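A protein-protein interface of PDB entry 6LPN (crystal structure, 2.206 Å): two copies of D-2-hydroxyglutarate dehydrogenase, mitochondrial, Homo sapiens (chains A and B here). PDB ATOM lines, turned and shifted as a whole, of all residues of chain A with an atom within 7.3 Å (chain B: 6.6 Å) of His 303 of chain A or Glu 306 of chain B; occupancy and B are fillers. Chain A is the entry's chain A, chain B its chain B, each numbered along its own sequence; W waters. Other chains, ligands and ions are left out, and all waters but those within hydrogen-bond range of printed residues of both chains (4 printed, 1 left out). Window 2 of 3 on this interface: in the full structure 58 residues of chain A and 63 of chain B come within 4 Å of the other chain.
Of the 12 printed residues of chain B, 4 touch a printed residue of chain A. Printed residues of chain B that touch a printed residue of chain A: Glu 259, His 303, Glu 306 and Lys 307. Hydrophobic or aromatic side chains of chain B that line the printed part of chain A: His 303. Of the 12 printed residues of chain A, 6 touch a printed residue of chain B. Hydrophobic or aromatic side chains of chain A that line the printed part of chain B: Ile 260 and His 303. Along chain A the printed residues that touch a printed residue of chain B span positions 260 to 307. Among the printed residues, no Asp or Glu carboxylate lies within 4 Å of a Lys or Arg side-chain nitrogen of the other chain.
A ring nitrogen (ND1) of His 303 of chain A is in hydrogen-bond range of the side-chain amino group (NZ) of Lys 307 of chain B (3.1 Å). OG of Ser 299 of chain A sits at hydrogen-bond distance from OE1 of Glu 259 of chain B. A ring nitrogen (NE2) of His 303 of chain A sits at hydrogen-bond distance from the side-chain carboxylate (OE1) of Glu 306 of chain B (3.0 Å). OE1 of Glu 306 of chain A is in hydrogen-bond range of NE2 of His 303 of chain B (2.9 Å). The side-chain amino group (NZ) of Lys 307 of chain A lies within hydrogen-bond range of a ring nitrogen (ND1) of His 303 of chain B.
Among the printed residues, merely in contact across the chains: Ile 260 of chain A with Glu 259 of chain B, Ser 299 of chain A with Lys 307 of chain B, Asn 300 of chain A with Lys 307 of chain B and His 303 of chain A with His 303 of chain B.
Water W2 lies within hydrogen-bond range of OE2 of Glu 259 of chain B (2.7 Å), NZ of Lys 307 of chain A (3.4 Å) and NZ of Lys 307 of chain B (3.4 Å). Water W1 lies within hydrogen-bond range of NZ of Lys 307 of chain B (2.7 Å), OD1 of Asp 304 of chain B (2.8 Å) and NZ of Lys 307 of chain A (3.4 Å). Water W4 bridges the side-chain carboxylate of Asp 304 of chain B (2.7 Å) and the side-chain amino group of Lys 307 of chain A (2.9 Å). Water W3 lies within hydrogen-bond range of the side-chain carboxylate of Glu 306 of chain A (2.8 Å) and the side-chain carboxylate of Glu 306 of chain B (3.0 Å).
The side-chain amino group (NZ) of Lys 307 of chain B is in salt-bridge range of the side-chain carboxylate (OE2) of Glu 259 of chain B (3.7 Å). The side-chain amide oxygen (OD1) of Asn 300 of chain A is in hydrogen-bond range of the backbone NH (N) of Gly 302 of chain A. The backbone NH (N) of His 303 of chain A lies within hydrogen-bond range of the side-chain amide oxygen (OD1) of Asn 300 of chain A (3.0 Å).
His 303 of chain A touches its own counterpart, His 303 of chain B. His 303 of chain A touches Glu 306 of chain B, and with the chains exchanged Glu 306 of chain A touches His 303 of chain B. His 303 of chain A touches Lys 307 of chain B, and with the chains exchanged Lys 307 of chain A touches His 303 of chain B. Positions printed for both chains: 301, 302, 303, 304, 305, 306, 307, 308 and 309. Of the 9 pairs that touch across the chains among the printed residues, 5 have their exchanged pair printed and touching as well.
Of the printed residues of chain B, Ser 299 of chain A touches Glu 259 (3.0 Å) and Lys 307 (3.3 Å). Printed residues of chain B within 4 Å of Asn 300 of chain A: Lys 307. His 303 of chain A touches just these residues of chain B: His 303, Glu 306 and Lys 307. Printed residues of chain B within 4 Å of Glu 306 of chain A: His 303. Of the printed residues of chain A, His 303 of chain B touches His 303, Glu 306 and Lys 307. No residue of chain A comes within 4 Å of Ala 305 of chain B. Of chain A, only His 303 comes within 4 Å of Glu 306 of chain B. Printed residues of chain A within 4 Å of Lys 307 of chain B: Ser 299 (3.3 Å), Asn 300 (3.8 Å) and His 303 (3.1 Å). The nearest residue of chain B that does not touch His 303 of chain A is Gly 302 of chain B (5.3 Å).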
ATOM      1  N   ILE A 260     -19.910 -18.381 -19.813  1.00  0.00           N
ATOM      2  CA  ILE A 260     -18.755 -19.190 -19.420  1.00  0.00           C
ATOM      3  C   ILE A 260     -17.533 -18.931 -20.288  1.00  0.00           C
ATOM      4  O   ILE A 260     -16.436 -19.375 -19.933  1.00  0.00           O
ATOM      5  CB  ILE A 260     -19.102 -20.692 -19.394  1.00  0.00           C
ATOM      6  CG1 ILE A 260     -19.373 -21.249 -20.793  1.00  0.00           C
ATOM      7  CG2 ILE A 260     -20.275 -20.970 -18.448  1.00  0.00           C
ATOM      8  CD1 ILE A 260     -19.433 -22.807 -20.819  1.00  0.00           C
ATOM      9  N   SER A 299     -18.696 -22.608 -13.011  1.00  0.00           N
ATOM     10  CA  SER A 299     -18.839 -23.156 -11.668  1.00  0.00           C
ATOM     11  C   SER A 299     -19.438 -24.550 -11.646  1.00  0.00           C
ATOM     12  O   SER A 299     -19.263 -25.267 -10.659  1.00  0.00           O
ATOM     13  CB  SER A 299     -19.708 -22.249 -10.796  1.00  0.00           C
ATOM     14  OG  SER A 299     -20.952 -22.017 -11.427  1.00  0.00           O
ATOM     15  N   ASN A 300     -20.148 -24.944 -12.698  1.00  0.00           N
ATOM     16  CA  ASN A 300     -20.715 -26.281 -12.817  1.00  0.00           C
ATOM     17  C   ASN A 300     -20.142 -26.943 -14.064  1.00  0.00           C
ATOM     18  O   ASN A 300     -20.489 -26.576 -15.196  1.00  0.00           O
ATOM     19  CB  ASN A 300     -22.245 -26.220 -12.855  1.00  0.00           C
ATOM     20  CG  ASN A 300     -22.897 -27.599 -12.814  1.00  0.00           C
ATOM     21  OD1 ASN A 300     -22.538 -28.492 -13.578  1.00  0.00           O
ATOM     22  ND2 ASN A 300     -23.857 -27.776 -11.910  1.00  0.00           N
ATOM     23  N   ALA A 301     -19.241 -27.904 -13.832  1.00  0.00           N
ATOM     24  CA  ALA A 301     -18.526 -28.573 -14.912  1.00  0.00           C
ATOM     25  C   ALA A 301     -19.483 -29.293 -15.847  1.00  0.00           C
ATOM     26  O   ALA A 301     -19.226 -29.395 -17.050  1.00  0.00           O
ATOM     27  CB  ALA A 301     -17.509 -29.559 -14.336  1.00  0.00           C
ATOM     28  N   GLY A 302     -20.562 -29.860 -15.304  1.00  0.00           N
ATOM     29  CA  GLY A 302     -21.506 -30.557 -16.160  1.00  0.00           C
ATOM     30  C   GLY A 302     -22.279 -29.627 -17.075  1.00  0.00           C
ATOM     31  O   GLY A 302     -22.459 -29.921 -18.260  1.00  0.00           O
ATOM     32  N   HIS A 303     -22.716 -28.476 -16.550  1.00  0.00           N
ATOM     33  CA  HIS A 303     -23.394 -27.492 -17.394  1.00  0.00           C
ATOM     34  C   HIS A 303     -22.462 -26.984 -18.481  1.00  0.00           C
ATOM     35  O   HIS A 303     -22.856 -26.874 -19.647  1.00  0.00           O
ATOM     36  CB  HIS A 303     -23.910 -26.318 -16.560  1.00  0.00           C
ATOM     37  CG  HIS A 303     -25.028 -26.681 -15.635  1.00  0.00           C
ATOM     38  ND1 HIS A 303     -25.232 -26.044 -14.431  1.00  0.00           N
ATOM     39  CD2 HIS A 303     -25.966 -27.653 -15.712  1.00  0.00           C
ATOM     40  CE1 HIS A 303     -26.270 -26.588 -13.821  1.00  0.00           C
ATOM     41  NE2 HIS A 303     -26.733 -27.567 -14.578  1.00  0.00           N
ATOM     42  N   ASP A 304     -21.208 -26.706 -18.127  1.00  0.00           N
ATOM     43  CA  ASP A 304     -20.237 -26.281 -19.128  1.00  0.00           C
ATOM     44  C   ASP A 304     -20.052 -27.350 -20.199  1.00  0.00           C
ATOM     45  O   ASP A 304     -20.076 -27.045 -21.394  1.00  0.00           O
ATOM     46  CB  ASP A 304     -18.900 -25.935 -18.473  1.00  0.00           C
ATOM     47  CG  ASP A 304     -18.988 -24.701 -17.557  1.00  0.00           C
ATOM     48  OD1 ASP A 304     -20.107 -24.177 -17.335  1.00  0.00           O
ATOM     49  OD2 ASP A 304     -17.924 -24.248 -17.078  1.00  0.00           O
ATOM     50  N   ALA A 305     -19.844 -28.608 -19.790  1.00  0.00           N
ATOM     51  CA  ALA A 305     -19.661 -29.684 -20.766  1.00  0.00           C
ATOM     52  C   ALA A 305     -20.862 -29.834 -21.703  1.00  0.00           C
ATOM     53  O   ALA A 305     -20.690 -30.071 -22.904  1.00  0.00           O
ATOM     54  CB  ALA A 305     -19.383 -31.009 -20.051  1.00  0.00           C
ATOM     55  N   GLU A 306     -22.084 -29.703 -21.179  1.00  0.00           N
ATOM     56  CA  GLU A 306     -23.260 -29.742 -22.050  1.00  0.00           C
ATOM     57  C   GLU A 306     -23.285 -28.573 -23.034  1.00  0.00           C
ATOM     58  O   GLU A 306     -23.603 -28.759 -24.219  1.00  0.00           O
ATOM     59  CB  GLU A 306     -24.534 -29.784 -21.203  1.00  0.00           C
ATOM     60  CG  GLU A 306     -24.773 -31.137 -20.514  1.00  0.00           C
ATOM     61  CD  GLU A 306     -26.090 -31.204 -19.742  1.00  0.00           C
ATOM     62  OE1 GLU A 306     -26.682 -30.140 -19.462  1.00  0.00           O
ATOM     63  OE2 GLU A 306     -26.545 -32.326 -19.430  1.00  0.00           O
ATOM     64  N   LYS A 307     -22.951 -27.363 -22.569  1.00  0.00           N
ATOM     65  CA  LYS A 307     -22.895 -26.210 -23.470  1.00  0.00           C
ATOM     66  C   LYS A 307     -21.867 -26.425 -24.571  1.00  0.00           C
ATOM     67  O   LYS A 307     -22.124 -26.142 -25.747  1.00  0.00           O
ATOM     68  CB  LYS A 307     -22.553 -24.936 -22.693  1.00  0.00           C
ATOM     69  CG  LYS A 307     -23.714 -24.303 -21.922  1.00  0.00           C
ATOM     70  CD  LYS A 307     -23.224 -23.026 -21.233  1.00  0.00           C
ATOM     71  CE  LYS A 307     -24.386 -22.250 -20.634  1.00  0.00           C
ATOM     72  NZ  LYS A 307     -24.709 -22.713 -19.244  1.00  0.00           N
ATOM     73  N   LEU A 308     -20.680 -26.898 -24.192  1.00  0.00           N
ATOM     74  CA  LEU A 308     -19.620 -27.178 -25.157  1.00  0.00           C
ATOM     75  C   LEU A 308     -20.048 -28.259 -26.141  1.00  0.00           C
ATOM     76  O   LEU A 308     -19.765 -28.166 -27.342  1.00  0.00           O
ATOM     77  CB  LEU A 308     -18.355 -27.571 -24.403  1.00  0.00           C
ATOM     78  CG  LEU A 308     -17.566 -26.303 -24.063  1.00  0.00           C
ATOM     79  CD1 LEU A 308     -16.539 -26.606 -22.997  1.00  0.00           C
ATOM     80  CD2 LEU A 308     -16.936 -25.648 -25.283  1.00  0.00           C
ATOM     81  N   GLY A 309     -20.682 -29.318 -25.635  1.00  0.00           N
ATOM     82  CA  GLY A 309     -21.165 -30.393 -26.491  1.00  0.00           C
ATOM     83  C   GLY A 309     -22.086 -29.895 -27.591  1.00  0.00           C
ATOM     84  O   GLY A 309     -21.914 -30.230 -28.765  1.00  0.00           O
ATOM     85  N   GLU B 259     -20.804 -17.744 -12.017  1.00  0.00           N
ATOM     86  CA  GLU B 259     -20.754 -16.756 -13.097  1.00  0.00           C
ATOM     87  C   GLU B 259     -22.123 -16.236 -13.556  1.00  0.00           C
ATOM     88  O   GLU B 259     -22.175 -15.203 -14.243  1.00  0.00           O
ATOM     89  CB  GLU B 259     -19.968 -17.329 -14.292  1.00  0.00           C
ATOM     90  CG  GLU B 259     -20.654 -18.437 -15.112  1.00  0.00           C
ATOM     91  CD  GLU B 259     -20.674 -19.809 -14.421  1.00  0.00           C
ATOM     92  OE1 GLU B 259     -20.018 -19.976 -13.366  1.00  0.00           O
ATOM     93  OE2 GLU B 259     -21.355 -20.723 -14.945  1.00  0.00           O
ATOM     94  N   ALA B 301     -31.372 -21.366 -20.193  1.00  0.00           N
ATOM     95  CA  ALA B 301     -32.451 -21.373 -19.209  1.00  0.00           C
ATOM     96  C   ALA B 301     -32.414 -22.622 -18.332  1.00  0.00           C
ATOM     97  O   ALA B 301     -32.463 -22.533 -17.101  1.00  0.00           O
ATOM     98  CB  ALA B 301     -33.801 -21.234 -19.923  1.00  0.00           C
ATOM     99  N   GLY B 302     -32.377 -23.802 -18.966  1.00  0.00           N
ATOM    100  CA  GLY B 302     -32.284 -25.060 -18.228  1.00  0.00           C
ATOM    101  C   GLY B 302     -31.155 -25.135 -17.217  1.00  0.00           C
ATOM    102  O   GLY B 302     -31.352 -25.559 -16.078  1.00  0.00           O
ATOM    103  N   HIS B 303     -29.951 -24.735 -17.618  1.00  0.00           N
ATOM    104  CA  HIS B 303     -28.821 -24.776 -16.689  1.00  0.00           C
ATOM    105  C   HIS B 303     -28.984 -23.788 -15.541  1.00  0.00           C
ATOM    106  O   HIS B 303     -28.717 -24.125 -14.379  1.00  0.00           O
ATOM    107  CB  HIS B 303     -27.518 -24.496 -17.421  1.00  0.00           C
ATOM    108  CG  HIS B 303     -27.181 -25.517 -18.456  1.00  0.00           C
ATOM    109  ND1 HIS B 303     -26.346 -25.251 -19.518  1.00  0.00           N
ATOM    110  CD2 HIS B 303     -27.542 -26.818 -18.575  1.00  0.00           C
ATOM    111  CE1 HIS B 303     -26.222 -26.338 -20.260  1.00  0.00           C
ATOM    112  NE2 HIS B 303     -26.935 -27.304 -19.708  1.00  0.00           N
ATOM    113  N   ASP B 304     -29.426 -22.572 -15.845  1.00  0.00           N
ATOM    114  CA  ASP B 304     -29.629 -21.582 -14.795  1.00  0.00           C
ATOM    115  C   ASP B 304     -30.690 -22.033 -13.796  1.00  0.00           C
ATOM    116  O   ASP B 304     -30.534 -21.830 -12.586  1.00  0.00           O
ATOM    117  CB  ASP B 304     -30.013 -20.240 -15.416  1.00  0.00           C
ATOM    118  CG  ASP B 304     -28.877 -19.621 -16.235  1.00  0.00           C
ATOM    119  OD1 ASP B 304     -27.841 -20.287 -16.464  1.00  0.00           O
ATOM    120  OD2 ASP B 304     -29.020 -18.448 -16.637  1.00  0.00           O
ATOM    121  N   ALA B 305     -31.770 -22.653 -14.279  1.00  0.00           N
ATOM    122  CA  ALA B 305     -32.792 -23.180 -13.378  1.00  0.00           C
ATOM    123  C   ALA B 305     -32.233 -24.273 -12.469  1.00  0.00           C
ATOM    124  O   ALA B 305     -32.550 -24.311 -11.272  1.00  0.00           O
ATOM    125  CB  ALA B 305     -33.985 -23.702 -14.183  1.00  0.00           C
ATOM    126  N   GLU B 306     -31.430 -25.192 -13.020  1.00  0.00           N
ATOM    127  CA  GLU B 306     -30.804 -26.212 -12.175  1.00  0.00           C
ATOM    128  C   GLU B 306     -29.877 -25.610 -11.122  1.00  0.00           C
ATOM    129  O   GLU B 306     -29.938 -25.990  -9.946  1.00  0.00           O
ATOM    130  CB  GLU B 306     -30.025 -27.205 -13.032  1.00  0.00           C
ATOM    131  CG  GLU B 306     -30.683 -28.529 -13.289  1.00  0.00           C
ATOM    132  CD  GLU B 306     -29.774 -29.435 -14.104  1.00  0.00           C
ATOM    133  OE1 GLU B 306     -28.652 -29.733 -13.632  1.00  0.00           O
ATOM    134  OE2 GLU B 306     -30.174 -29.838 -15.218  1.00  0.00           O
ATOM    135  N   LYS B 307     -29.010 -24.675 -11.517  1.00  0.00           N
ATOM    136  CA  LYS B 307     -28.163 -24.004 -10.531  1.00  0.00           C
ATOM    137  C   LYS B 307     -28.996 -23.344  -9.432  1.00  0.00           C
ATOM    138  O   LYS B 307     -28.741 -23.542  -8.239  1.00  0.00           O
ATOM    139  CB  LYS B 307     -27.283 -22.955 -11.212  1.00  0.00           C
ATOM    140  CG  LYS B 307     -26.057 -23.463 -11.919  1.00  0.00           C
ATOM    141  CD  LYS B 307     -25.171 -22.273 -12.328  1.00  0.00           C
ATOM    142  CE  LYS B 307     -23.858 -22.730 -12.930  1.00  0.00           C
ATOM    143  NZ  LYS B 307     -24.027 -23.186 -14.354  1.00  0.00           N
ATOM    144  N   LEU B 308     -30.020 -22.578  -9.824  1.00  0.00           N
ATOM    145  CA  LEU B 308     -30.878 -21.902  -8.852  1.00  0.00           C
ATOM    146  C   LEU B 308     -31.659 -22.882  -7.976  1.00  0.00           C
ATOM    147  O   LEU B 308     -31.790 -22.666  -6.765  1.00  0.00           O
ATOM    148  CB  LEU B 308     -31.823 -20.953  -9.587  1.00  0.00           C
ATOM    149  CG  LEU B 308     -32.430 -19.805  -8.777  1.00  0.00           C
ATOM    150  CD1 LEU B 308     -31.336 -18.897  -8.225  1.00  0.00           C
ATOM    151  CD2 LEU B 308     -33.396 -19.017  -9.644  1.00  0.00           C
ATOM    152  N   GLY B 309     -32.224 -23.934  -8.574  1.00  0.00           N
ATOM    153  CA  GLY B 309     -32.941 -24.939  -7.793  1.00  0.00           C
ATOM    154  C   GLY B 309     -32.112 -25.566  -6.682  1.00  0.00           C
ATOM    155  O   GLY B 309     -32.555 -25.665  -5.530  1.00  0.00           O
ATOM    156  N   HIS B 310     -30.888 -25.977  -7.011  1.00  0.00           N
ATOM    157  CA  HIS B 310     -29.993 -26.559  -6.015  1.00  0.00           C
ATOM    158  C   HIS B 310     -29.597 -25.528  -4.967  1.00  0.00           C
ATOM    159  O   HIS B 310     -29.477 -25.857  -3.777  1.00  0.00           O
ATOM    160  CB  HIS B 310     -28.760 -27.153  -6.701  1.00  0.00           C
ATOM    161  CG  HIS B 310     -27.979 -28.096  -5.836  1.00  0.00           C
ATOM    162  ND1 HIS B 310     -28.548 -28.801  -4.794  1.00  0.00           N
ATOM    163  CD2 HIS B 310     -26.677 -28.471  -5.875  1.00  0.00           C
ATOM    164  CE1 HIS B 310     -27.627 -29.555  -4.220  1.00  0.00           C
ATOM    165  NE2 HIS B 310     -26.484 -29.374  -4.857  1.00  0.00           N
ATOM    166  N   PHE B 311     -29.340 -24.291  -5.395  1.00  0.00           N
ATOM    167  CA  PHE B 311     -29.015 -23.227  -4.452  1.00  0.00           C
ATOM    168  C   PHE B 311     -30.118 -23.018  -3.421  1.00  0.00           C
ATOM    169  O   PHE B 311     -29.843 -22.921  -2.219  1.00  0.00           O
ATOM    170  CB  PHE B 311     -28.772 -21.918  -5.197  1.00  0.00           C
ATOM    171  CG  PHE B 311     -28.865 -20.722  -4.315  1.00  0.00           C
ATOM    172  CD1 PHE B 311     -27.875 -20.434  -3.385  1.00  0.00           C
ATOM    173  CD2 PHE B 311     -29.982 -19.891  -4.384  1.00  0.00           C
ATOM    174  CE1 PHE B 311     -27.990 -19.312  -2.550  1.00  0.00           C
ATOM    175  CE2 PHE B 311     -30.099 -18.777  -3.561  1.00  0.00           C
ATOM    176  CZ  PHE B 311     -29.096 -18.493  -2.643  1.00  0.00           C
HETATM  177  O   HOH W   1     -25.749 -22.040 -16.118  1.00  0.00           O
HETATM  178  O   HOH W   2     -23.338 -20.858 -16.758  1.00  0.00           O
HETATM  179  O   HOH W   3     -28.948 -30.363 -17.896  1.00  0.00           O
HETATM  180  O   HOH W   4     -26.434 -20.413 -18.807  1.00  0.00           O
